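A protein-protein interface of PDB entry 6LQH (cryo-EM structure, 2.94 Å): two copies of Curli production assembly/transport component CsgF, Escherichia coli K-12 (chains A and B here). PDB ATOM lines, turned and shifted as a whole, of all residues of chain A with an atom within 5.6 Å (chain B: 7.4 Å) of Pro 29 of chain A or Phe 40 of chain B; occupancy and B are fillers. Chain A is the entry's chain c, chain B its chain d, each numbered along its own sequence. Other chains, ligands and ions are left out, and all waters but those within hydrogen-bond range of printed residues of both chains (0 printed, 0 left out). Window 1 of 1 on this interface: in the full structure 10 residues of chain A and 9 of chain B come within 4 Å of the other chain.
N of Gly 32 of chain A sits close to NE of Arg 27 of chain B, 3.0 Å away.
The backbone carbonyl oxygen of Arg 27 of chain B sits close to the side-chain amide nitrogen of Asn 37 of chain B (3.3 Å).
The backbone carbonyl oxygen of Leu 41 of chain B lies within hydrogen-bond range of the side-chain hydroxyl of Ser 44 of chain B (3.4 Å).
OD1 of Asn 34 of chain A sits close to N of Asn 36 of chain A (3.5 Å).
Pro 29 of chain A touches Asn 37 of chain B.
Pro 29 of chain A touches Phe 40 of chain B.
Phe 40 of chain B touches Asn 30 of chain A (CE2 to ND2, 3.4 Å).
Leu 41 of chain B touches Asn 30 of chain A (CD2 to OD1, 3.3 Å).
CA of Phe 31 of chain A touches NE of Arg 27 of chain B, at 3.3 Å.
CB of Asn 36 of chain B touches CB of Pro 35 of chain A (3.5 Å).
Asn 37 of chain B touches Pro 35 of chain A.
Asn 36 of chain A touches Asn 36 of chain B (OD1 to ND2, 3.8 Å).
Leu 42 of chain A touches Phe 40 of chain B (CB to CE1, 3.7 Å).
Leu 42 of chain A touches Ser 44 of chain B (CD1 to CA, 3.6 Å).
Of chain B, only Asn 37 (3.3 Å) and Phe 40 (3.4 Å) come within 4 Å of Pro 29 of chain A.
Printed residues of chain B within 4 Å of Asn 30 of chain A: Phe 40 (3.4 Å) and Leu 41 (3.3 Å).
Ala 39 of chain A touches none of the printed residues of chain B.
Printed residues of chain A within 4 Å of Arg 27 of chain B: Phe 31 (3.3 Å) and Gly 32 (3.0 Å).
Of the printed residues of chain A, Asn 36 of chain B touches Pro 35 and Asn 36.
Of the printed residues of chain A, Asn 37 of chain B touches Pro 29 (3.3 Å) and Pro 35 (3.1 Å).
Phe 40 of chain B touches just these residues of chain A: Pro 29 (3.4 Å), Asn 30 (3.4 Å), Gly 38 (3.0 Å) and Leu 42 (3.7 Å).
Of the printed residues of chain A, Leu 41 of chain B touches Asn 30 (3.3 Å).
Leu 42 of chain B touches none of the printed residues of chain A.
The nearest printed residue of chain A that does not touch Asn 37 of chain B is Gly 33 of chain A (4.3 Å).
Printed residues of chain A that touch a printed residue of chain B: Pro 29, Asn 30, Phe 31, Gly 32, Pro 35, Asn 36, Gly 38 and Leu 42.
Hydrophobic or aromatic side chains of chain A within 4 Å of the printed part of chain B: Pro 29, Pro 35 and Leu 42.
Of the 14 printed residues of chain B, 7 touch a printed residue of chain A.
Printed residues of chain B that touch a printed residue of chain A: Arg 27, Asn 36, Asn 37, Phe 40, Leu 41, Asn 43 and Ser 44.
Along chain B the printed residues that touch a printed residue of chain A span positions 27 to 44.
Among the printed residues, no Asp or Glu carboxylate lies within 4 Å of a Lys or Arg side-chain nitrogen of the other chain.
Pro 35 of chain A touches Asn 36 of chain B, but with the chains exchanged Asn 36 of chain A does not touch Pro 35 of chain B (8.1 Å).
Pro 35 of chain A touches Asn 37 of chain B, but with the chains exchanged Asn 37 of chain A does not touch Pro 35 of chain B (11.0 Å).
Asn 36 of chain A touches its own counterpart, Asn 36 of chain B.
Positions printed for both chains: 27, 28, 35, 36, 37, 38, 39, 41 and 42.
Of the 13 pairs that touch across the chains among the printed residues, 1 has its exchanged pair printed and touching as well.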
ATOM      1  N   ARG A  27      21.002  24.018  13.016  1.00  0.00           N
ATOM      2  CA  ARG A  27      20.932  24.099  14.470  1.00  0.00           C
ATOM      3  C   ARG A  27      22.204  24.682  15.064  1.00  0.00           C
ATOM      4  O   ARG A  27      22.146  25.374  16.085  1.00  0.00           O
ATOM      5  CB  ARG A  27      20.683  22.719  15.072  1.00  0.00           C
ATOM      6  CG  ARG A  27      19.627  21.905  14.362  1.00  0.00           C
ATOM      7  CD  ARG A  27      18.240  22.408  14.654  1.00  0.00           C
ATOM      8  NE  ARG A  27      17.254  21.377  14.361  1.00  0.00           N
ATOM      9  CZ  ARG A  27      16.265  21.514  13.489  1.00  0.00           C
ATOM     10  NH1 ARG A  27      16.118  22.650  12.824  1.00  0.00           N
ATOM     11  NH2 ARG A  27      15.416  20.516  13.292  1.00  0.00           N
ATOM     12  N   ASN A  28      23.352  24.409  14.455  1.00  0.00           N
ATOM     13  CA  ASN A  28      24.597  24.943  14.975  1.00  0.00           C
ATOM     14  C   ASN A  28      24.729  26.425  14.649  1.00  0.00           C
ATOM     15  O   ASN A  28      24.347  26.867  13.562  1.00  0.00           O
ATOM     16  CB  ASN A  28      25.795  24.201  14.386  1.00  0.00           C
ATOM     17  CG  ASN A  28      25.959  22.803  14.936  1.00  0.00           C
ATOM     18  OD1 ASN A  28      25.294  22.416  15.891  1.00  0.00           O
ATOM     19  ND2 ASN A  28      26.868  22.046  14.347  1.00  0.00           N
ATOM     20  N   PRO A  29      25.257  27.215  15.585  1.00  0.00           N
ATOM     21  CA  PRO A  29      25.719  28.557  15.217  1.00  0.00           C
ATOM     22  C   PRO A  29      26.893  28.512  14.269  1.00  0.00           C
ATOM     23  O   PRO A  29      26.978  29.345  13.357  1.00  0.00           O
ATOM     24  CB  PRO A  29      26.102  29.179  16.562  1.00  0.00           C
ATOM     25  CG  PRO A  29      26.377  28.035  17.431  1.00  0.00           C
ATOM     26  CD  PRO A  29      25.464  26.935  17.011  1.00  0.00           C
ATOM     27  N   ASN A  30      27.808  27.566  14.463  1.00  0.00           N
ATOM     28  CA  ASN A  30      28.742  27.224  13.406  1.00  0.00           C
ATOM     29  C   ASN A  30      27.955  26.831  12.168  1.00  0.00           C
ATOM     30  O   ASN A  30      27.036  26.013  12.234  1.00  0.00           O
ATOM     31  CB  ASN A  30      29.651  26.074  13.832  1.00  0.00           C
ATOM     32  CG  ASN A  30      30.663  26.487  14.873  1.00  0.00           C
ATOM     33  OD1 ASN A  30      31.031  27.656  14.967  1.00  0.00           O
ATOM     34  ND2 ASN A  30      31.119  25.526  15.665  1.00  0.00           N
ATOM     35  N   PHE A  31      28.309  27.436  11.043  1.00  0.00           N
ATOM     36  CA  PHE A  31      27.648  27.193   9.768  1.00  0.00           C
ATOM     37  C   PHE A  31      26.121  27.210   9.845  1.00  0.00           C
ATOM     38  O   PHE A  31      25.476  26.172   9.706  1.00  0.00           O
ATOM     39  CB  PHE A  31      28.157  25.899   9.096  1.00  0.00           C
ATOM     40  CG  PHE A  31      28.123  24.642   9.942  1.00  0.00           C
ATOM     41  CD1 PHE A  31      26.978  23.868  10.035  1.00  0.00           C
ATOM     42  CD2 PHE A  31      29.274  24.179  10.551  1.00  0.00           C
ATOM     43  CE1 PHE A  31      26.963  22.712  10.778  1.00  0.00           C
ATOM     44  CE2 PHE A  31      29.259  23.017  11.289  1.00  0.00           C
ATOM     45  CZ  PHE A  31      28.104  22.284  11.401  1.00  0.00           C
ATOM     46  N   GLY A  32      25.526  28.381  10.058  1.00  0.00           N
ATOM     47  CA  GLY A  32      24.097  28.476   9.834  1.00  0.00           C
ATOM     48  C   GLY A  32      23.225  29.362  10.700  1.00  0.00           C
ATOM     49  O   GLY A  32      22.006  29.385  10.504  1.00  0.00           O
ATOM     50  N   GLY A  33      23.799  30.104  11.640  1.00  0.00           N
ATOM     51  CA  GLY A  33      23.125  31.319  12.055  1.00  0.00           C
ATOM     52  C   GLY A  33      22.618  31.508  13.471  1.00  0.00           C
ATOM     53  O   GLY A  33      22.773  32.607  14.009  1.00  0.00           O
ATOM     54  N   ASN A  34      21.999  30.499  14.090  1.00  0.00           N
ATOM     55  CA  ASN A  34      21.397  30.754  15.394  1.00  0.00           C
ATOM     56  C   ASN A  34      22.453  30.606  16.479  1.00  0.00           C
ATOM     57  O   ASN A  34      22.911  29.486  16.743  1.00  0.00           O
ATOM     58  CB  ASN A  34      20.215  29.820  15.657  1.00  0.00           C
ATOM     59  CG  ASN A  34      19.321  30.314  16.787  1.00  0.00           C
ATOM     60  OD1 ASN A  34      19.752  31.069  17.653  1.00  0.00           O
ATOM     61  ND2 ASN A  34      18.063  29.893  16.772  1.00  0.00           N
ATOM     62  N   PRO A  35      22.861  31.686  17.140  1.00  0.00           N
ATOM     63  CA  PRO A  35      24.032  31.618  18.022  1.00  0.00           C
ATOM     64  C   PRO A  35      23.719  31.135  19.426  1.00  0.00           C
ATOM     65  O   PRO A  35      24.622  30.702  20.147  1.00  0.00           O
ATOM     66  CB  PRO A  35      24.541  33.067  18.036  1.00  0.00           C
ATOM     67  CG  PRO A  35      23.619  33.847  17.110  1.00  0.00           C
ATOM     68  CD  PRO A  35      22.364  33.060  17.017  1.00  0.00           C
ATOM     69  N   ASN A  36      22.454  31.217  19.836  1.00  0.00           N
ATOM     70  CA  ASN A  36      22.110  30.838  21.202  1.00  0.00           C
ATOM     71  C   ASN A  36      22.226  29.334  21.408  1.00  0.00           C
ATOM     72  O   ASN A  36      22.359  28.866  22.545  1.00  0.00           O
ATOM     73  CB  ASN A  36      20.703  31.318  21.548  1.00  0.00           C
ATOM     74  CG  ASN A  36      20.541  32.807  21.382  1.00  0.00           C
ATOM     75  OD1 ASN A  36      21.330  33.456  20.699  1.00  0.00           O
ATOM     76  ND2 ASN A  36      19.512  33.361  22.006  1.00  0.00           N
ATOM     77  N   ASN A  37      22.183  28.559  20.323  1.00  0.00           N
ATOM     78  CA  ASN A  37      22.271  27.108  20.452  1.00  0.00           C
ATOM     79  C   ASN A  37      23.662  26.668  20.885  1.00  0.00           C
ATOM     80  O   ASN A  37      23.814  25.619  21.518  1.00  0.00           O
ATOM     81  CB  ASN A  37      21.894  26.429  19.137  1.00  0.00           C
ATOM     82  CG  ASN A  37      20.439  26.601  18.788  1.00  0.00           C
ATOM     83  OD1 ASN A  37      19.562  26.039  19.438  1.00  0.00           O
ATOM     84  ND2 ASN A  37      20.170  27.374  17.749  1.00  0.00           N
ATOM     85  N   GLY A  38      24.687  27.450  20.544  1.00  0.00           N
ATOM     86  CA  GLY A  38      26.052  26.988  20.733  1.00  0.00           C
ATOM     87  C   GLY A  38      26.447  26.855  22.188  1.00  0.00           C
ATOM     88  O   GLY A  38      27.201  25.950  22.556  1.00  0.00           O
ATOM     89  N   ALA A  39      25.955  27.759  23.036  1.00  0.00           N
ATOM     90  CA  ALA A  39      26.271  27.670  24.457  1.00  0.00           C
ATOM     91  C   ALA A  39      25.819  26.337  25.030  1.00  0.00           C
ATOM     92  O   ALA A  39      26.574  25.674  25.748  1.00  0.00           O
ATOM     93  CB  ALA A  39      25.627  28.830  25.212  1.00  0.00           C
ATOM     94  N   LEU A  41      25.103  23.648  23.189  1.00  0.00           N
ATOM     95  CA  LEU A  41      25.698  22.567  22.413  1.00  0.00           C
ATOM     96  C   LEU A  41      27.067  22.189  22.950  1.00  0.00           C
ATOM     97  O   LEU A  41      27.356  21.004  23.155  1.00  0.00           O
ATOM     98  CB  LEU A  41      25.799  22.980  20.948  1.00  0.00           C
ATOM     99  CG  LEU A  41      24.591  22.622  20.091  1.00  0.00           C
ATOM    100  CD1 LEU A  41      24.660  23.359  18.779  1.00  0.00           C
ATOM    101  CD2 LEU A  41      24.529  21.123  19.865  1.00  0.00           C
ATOM    102  N   LEU A  42      27.925  23.181  23.190  1.00  0.00           N
ATOM    103  CA  LEU A  42      29.257  22.879  23.700  1.00  0.00           C
ATOM    104  C   LEU A  42      29.199  22.307  25.109  1.00  0.00           C
ATOM    105  O   LEU A  42      29.988  21.419  25.447  1.00  0.00           O
ATOM    106  CB  LEU A  42      30.136  24.127  23.664  1.00  0.00           C
ATOM    107  CG  LEU A  42      31.556  23.916  24.187  1.00  0.00           C
ATOM    108  CD1 LEU A  42      32.482  23.510  23.061  1.00  0.00           C
ATOM    109  CD2 LEU A  42      32.060  25.163  24.878  1.00  0.00           C
ATOM    110  N   ARG B  27      29.758  34.399  10.035  1.00  0.00           N
ATOM    111  CA  ARG B  27      29.454  33.726  11.292  1.00  0.00           C
ATOM    112  C   ARG B  27      30.208  34.342  12.460  1.00  0.00           C
ATOM    113  O   ARG B  27      29.691  34.372  13.580  1.00  0.00           O
ATOM    114  CB  ARG B  27      29.795  32.241  11.201  1.00  0.00           C
ATOM    115  CG  ARG B  27      29.353  31.573   9.920  1.00  0.00           C
ATOM    116  CD  ARG B  27      27.867  31.348   9.887  1.00  0.00           C
ATOM    117  NE  ARG B  27      27.527  30.327   8.907  1.00  0.00           N
ATOM    118  CZ  ARG B  27      26.723  30.521   7.871  1.00  0.00           C
ATOM    119  NH1 ARG B  27      26.158  31.704   7.681  1.00  0.00           N
ATOM    120  NH2 ARG B  27      26.475  29.526   7.032  1.00  0.00           N
ATOM    121  N   ASN B  28      31.423  34.822  12.225  1.00  0.00           N
ATOM    122  CA  ASN B  28      32.188  35.424  13.300  1.00  0.00           C
ATOM    123  C   ASN B  28      31.657  36.815  13.628  1.00  0.00           C
ATOM    124  O   ASN B  28      31.272  37.569  12.731  1.00  0.00           O
ATOM    125  CB  ASN B  28      33.664  35.538  12.921  1.00  0.00           C
ATOM    126  CG  ASN B  28      34.380  34.208  12.919  1.00  0.00           C
ATOM    127  OD1 ASN B  28      33.847  33.198  13.367  1.00  0.00           O
ATOM    128  ND2 ASN B  28      35.613  34.208  12.437  1.00  0.00           N
ATOM    129  N   PRO B  35      27.220  39.145  17.128  1.00  0.00           N
ATOM    130  CA  PRO B  35      28.150  39.065  18.259  1.00  0.00           C
ATOM    131  C   PRO B  35      27.904  37.881  19.176  1.00  0.00           C
ATOM    132  O   PRO B  35      28.792  37.494  19.940  1.00  0.00           O
ATOM    133  CB  PRO B  35      27.916  40.391  18.998  1.00  0.00           C
ATOM    134  CG  PRO B  35      26.878  41.149  18.181  1.00  0.00           C
ATOM    135  CD  PRO B  35      26.163  40.130  17.374  1.00  0.00           C
ATOM    136  N   ASN B  36      26.702  37.305  19.128  1.00  0.00           N
ATOM    137  CA  ASN B  36      26.387  36.213  20.040  1.00  0.00           C
ATOM    138  C   ASN B  36      27.161  34.949  19.686  1.00  0.00           C
ATOM    139  O   ASN B  36      27.334  34.064  20.532  1.00  0.00           O
ATOM    140  CB  ASN B  36      24.885  35.937  20.039  1.00  0.00           C
ATOM    141  CG  ASN B  36      24.072  37.151  20.405  1.00  0.00           C
ATOM    142  OD1 ASN B  36      24.556  38.279  20.335  1.00  0.00           O
ATOM    143  ND2 ASN B  36      22.828  36.929  20.801  1.00  0.00           N
ATOM    144  N   ASN B  37      27.637  34.848  18.444  1.00  0.00           N
ATOM    145  CA  ASN B  37      28.374  33.657  18.034  1.00  0.00           C
ATOM    146  C   ASN B  37      29.732  33.576  18.715  1.00  0.00           C
ATOM    147  O   ASN B  37      30.265  32.480  18.913  1.00  0.00           O
ATOM    148  CB  ASN B  37      28.547  33.629  16.517  1.00  0.00           C
ATOM    149  CG  ASN B  37      27.245  33.432  15.785  1.00  0.00           C
ATOM    150  OD1 ASN B  37      26.650  32.359  15.830  1.00  0.00           O
ATOM    151  ND2 ASN B  37      26.797  34.467  15.094  1.00  0.00           N
ATOM    152  N   GLY B  38      30.311  34.725  19.069  1.00  0.00           N
ATOM    153  CA  GLY B  38      31.691  34.737  19.522  1.00  0.00           C
ATOM    154  C   GLY B  38      31.892  34.053  20.859  1.00  0.00           C
ATOM    155  O   GLY B  38      32.922  33.412  21.088  1.00  0.00           O
ATOM    156  N   ALA B  39      30.922  34.188  21.762  1.00  0.00           N
ATOM    157  CA  ALA B  39      31.038  33.529  23.057  1.00  0.00           C
ATOM    158  C   ALA B  39      31.184  32.025  22.891  1.00  0.00           C
ATOM    159  O   ALA B  39      32.052  31.405  23.514  1.00  0.00           O
ATOM    160  CB  ALA B  39      29.828  33.861  23.928  1.00  0.00           C
ATOM    161  N   PHE B  40      30.362  31.426  22.030  1.00  0.00           N
ATOM    162  CA  PHE B  40      30.463  29.992  21.789  1.00  0.00           C
ATOM    163  C   PHE B  40      31.701  29.656  20.975  1.00  0.00           C
ATOM    164  O   PHE B  40      32.317  28.605  21.178  1.00  0.00           O
ATOM    165  CB  PHE B  40      29.210  29.493  21.074  1.00  0.00           C
ATOM    166  CG  PHE B  40      29.407  28.199  20.341  1.00  0.00           C
ATOM    167  CD1 PHE B  40      29.554  27.013  21.032  1.00  0.00           C
ATOM    168  CD2 PHE B  40      29.449  28.171  18.962  1.00  0.00           C
ATOM    169  CE1 PHE B  40      29.730  25.822  20.361  1.00  0.00           C
ATOM    170  CE2 PHE B  40      29.627  26.982  18.289  1.00  0.00           C
ATOM    171  CZ  PHE B  40      29.767  25.809  18.989  1.00  0.00           C
ATOM    172  N   LEU B  41      32.074  30.533  20.042  1.00  0.00           N
ATOM    173  CA  LEU B  41      33.208  30.258  19.167  1.00  0.00           C
ATOM    174  C   LEU B  41      34.504  30.166  19.954  1.00  0.00           C
ATOM    175  O   LEU B  41      35.280  29.221  19.779  1.00  0.00           O
ATOM    176  CB  LEU B  41      33.310  31.342  18.100  1.00  0.00           C
ATOM    177  CG  LEU B  41      32.544  31.056  16.814  1.00  0.00           C
ATOM    178  CD1 LEU B  41      32.446  32.314  15.990  1.00  0.00           C
ATOM    179  CD2 LEU B  41      33.222  29.950  16.029  1.00  0.00           C
ATOM    180  N   LEU B  42      34.757  31.140  20.830  1.00  0.00           N
ATOM    181  CA  LEU B  42      35.988  31.111  21.610  1.00  0.00           C
ATOM    182  C   LEU B  42      36.007  29.942  22.584  1.00  0.00           C
ATOM    183  O   LEU B  42      37.060  29.340  22.808  1.00  0.00           O
ATOM    184  CB  LEU B  42      36.178  32.431  22.353  1.00  0.00           C
ATOM    185  CG  LEU B  42      37.442  32.499  23.208  1.00  0.00           C
ATOM    186  CD1 LEU B  42      38.599  33.049  22.403  1.00  0.00           C
ATOM    187  CD2 LEU B  42      37.203  33.331  24.447  1.00  0.00           C
ATOM    188  N   ASN B  43      34.854  29.593  23.157  1.00  0.00           N
ATOM    189  CA  ASN B  43      34.804  28.460  24.074  1.00  0.00           C
ATOM    190  C   ASN B  43      35.057  27.144  23.354  1.00  0.00           C
ATOM    191  O   ASN B  43      35.771  26.278  23.870  1.00  0.00           O
ATOM    192  CB  ASN B  43      33.457  28.417  24.793  1.00  0.00           C
ATOM    193  CG  ASN B  43      33.211  29.641  25.639  1.00  0.00           C
ATOM    194  OD1 ASN B  43      34.079  30.065  26.398  1.00  0.00           O
ATOM    195  ND2 ASN B  43      32.018  30.204  25.533  1.00  0.00           N
ATOM    196  N   SER B  44      34.481  26.971  22.166  1.00  0.00           N
ATOM    197  CA  SER B  44      34.699  25.751  21.406  1.00  0.00           C
ATOM    198  C   SER B  44      36.085  25.691  20.782  1.00  0.00           C
ATOM    199  O   SER B  44      36.562  24.596  20.469  1.00  0.00           O
ATOM    200  CB  SER B  44      33.622  25.606  20.328  1.00  0.00           C
ATOM    201  OG  SER B  44      34.053  26.142  19.092  1.00  0.00           O
ATOM    202  N   ALA B  45      36.737  26.834  20.594  1.00  0.00           N
ATOM    203  CA  ALA B  45      38.133  26.842  20.183  1.00  0.00           C
ATOM    204  C   ALA B  45      39.074  26.588  21.347  1.00  0.00           C
ATOM    205  O   ALA B  45      40.179  26.073  21.141  1.00  0.00           O
ATOM    206  CB  ALA B  45      38.484  28.175  19.521  1.00  0.00           C
ATOM    207  N   GLN B  46      38.664  26.944  22.562  1.00  0.00           N
ATOM    208  CA  GLN B  46      39.429  26.625  23.757  1.00  0.00           C
ATOM    209  C   GLN B  46      39.164  25.217  24.260  1.00  0.00           C
ATOM    210  O   GLN B  46      40.019  24.644  24.944  1.00  0.00           O
ATOM    211  CB  GLN B  46      39.121  27.628  24.871  1.00  0.00           C
ATOM    212  CG  GLN B  46      39.722  29.000  24.655  1.00  0.00           C
ATOM    213  CD  GLN B  46      41.169  29.085  25.099  1.00  0.00           C
ATOM    214  OE1 GLN B  46      41.840  28.070  25.272  1.00  0.00           O
ATOM    215  NE2 GLN B  46      41.654  30.303  25.289  1.00  0.00           N
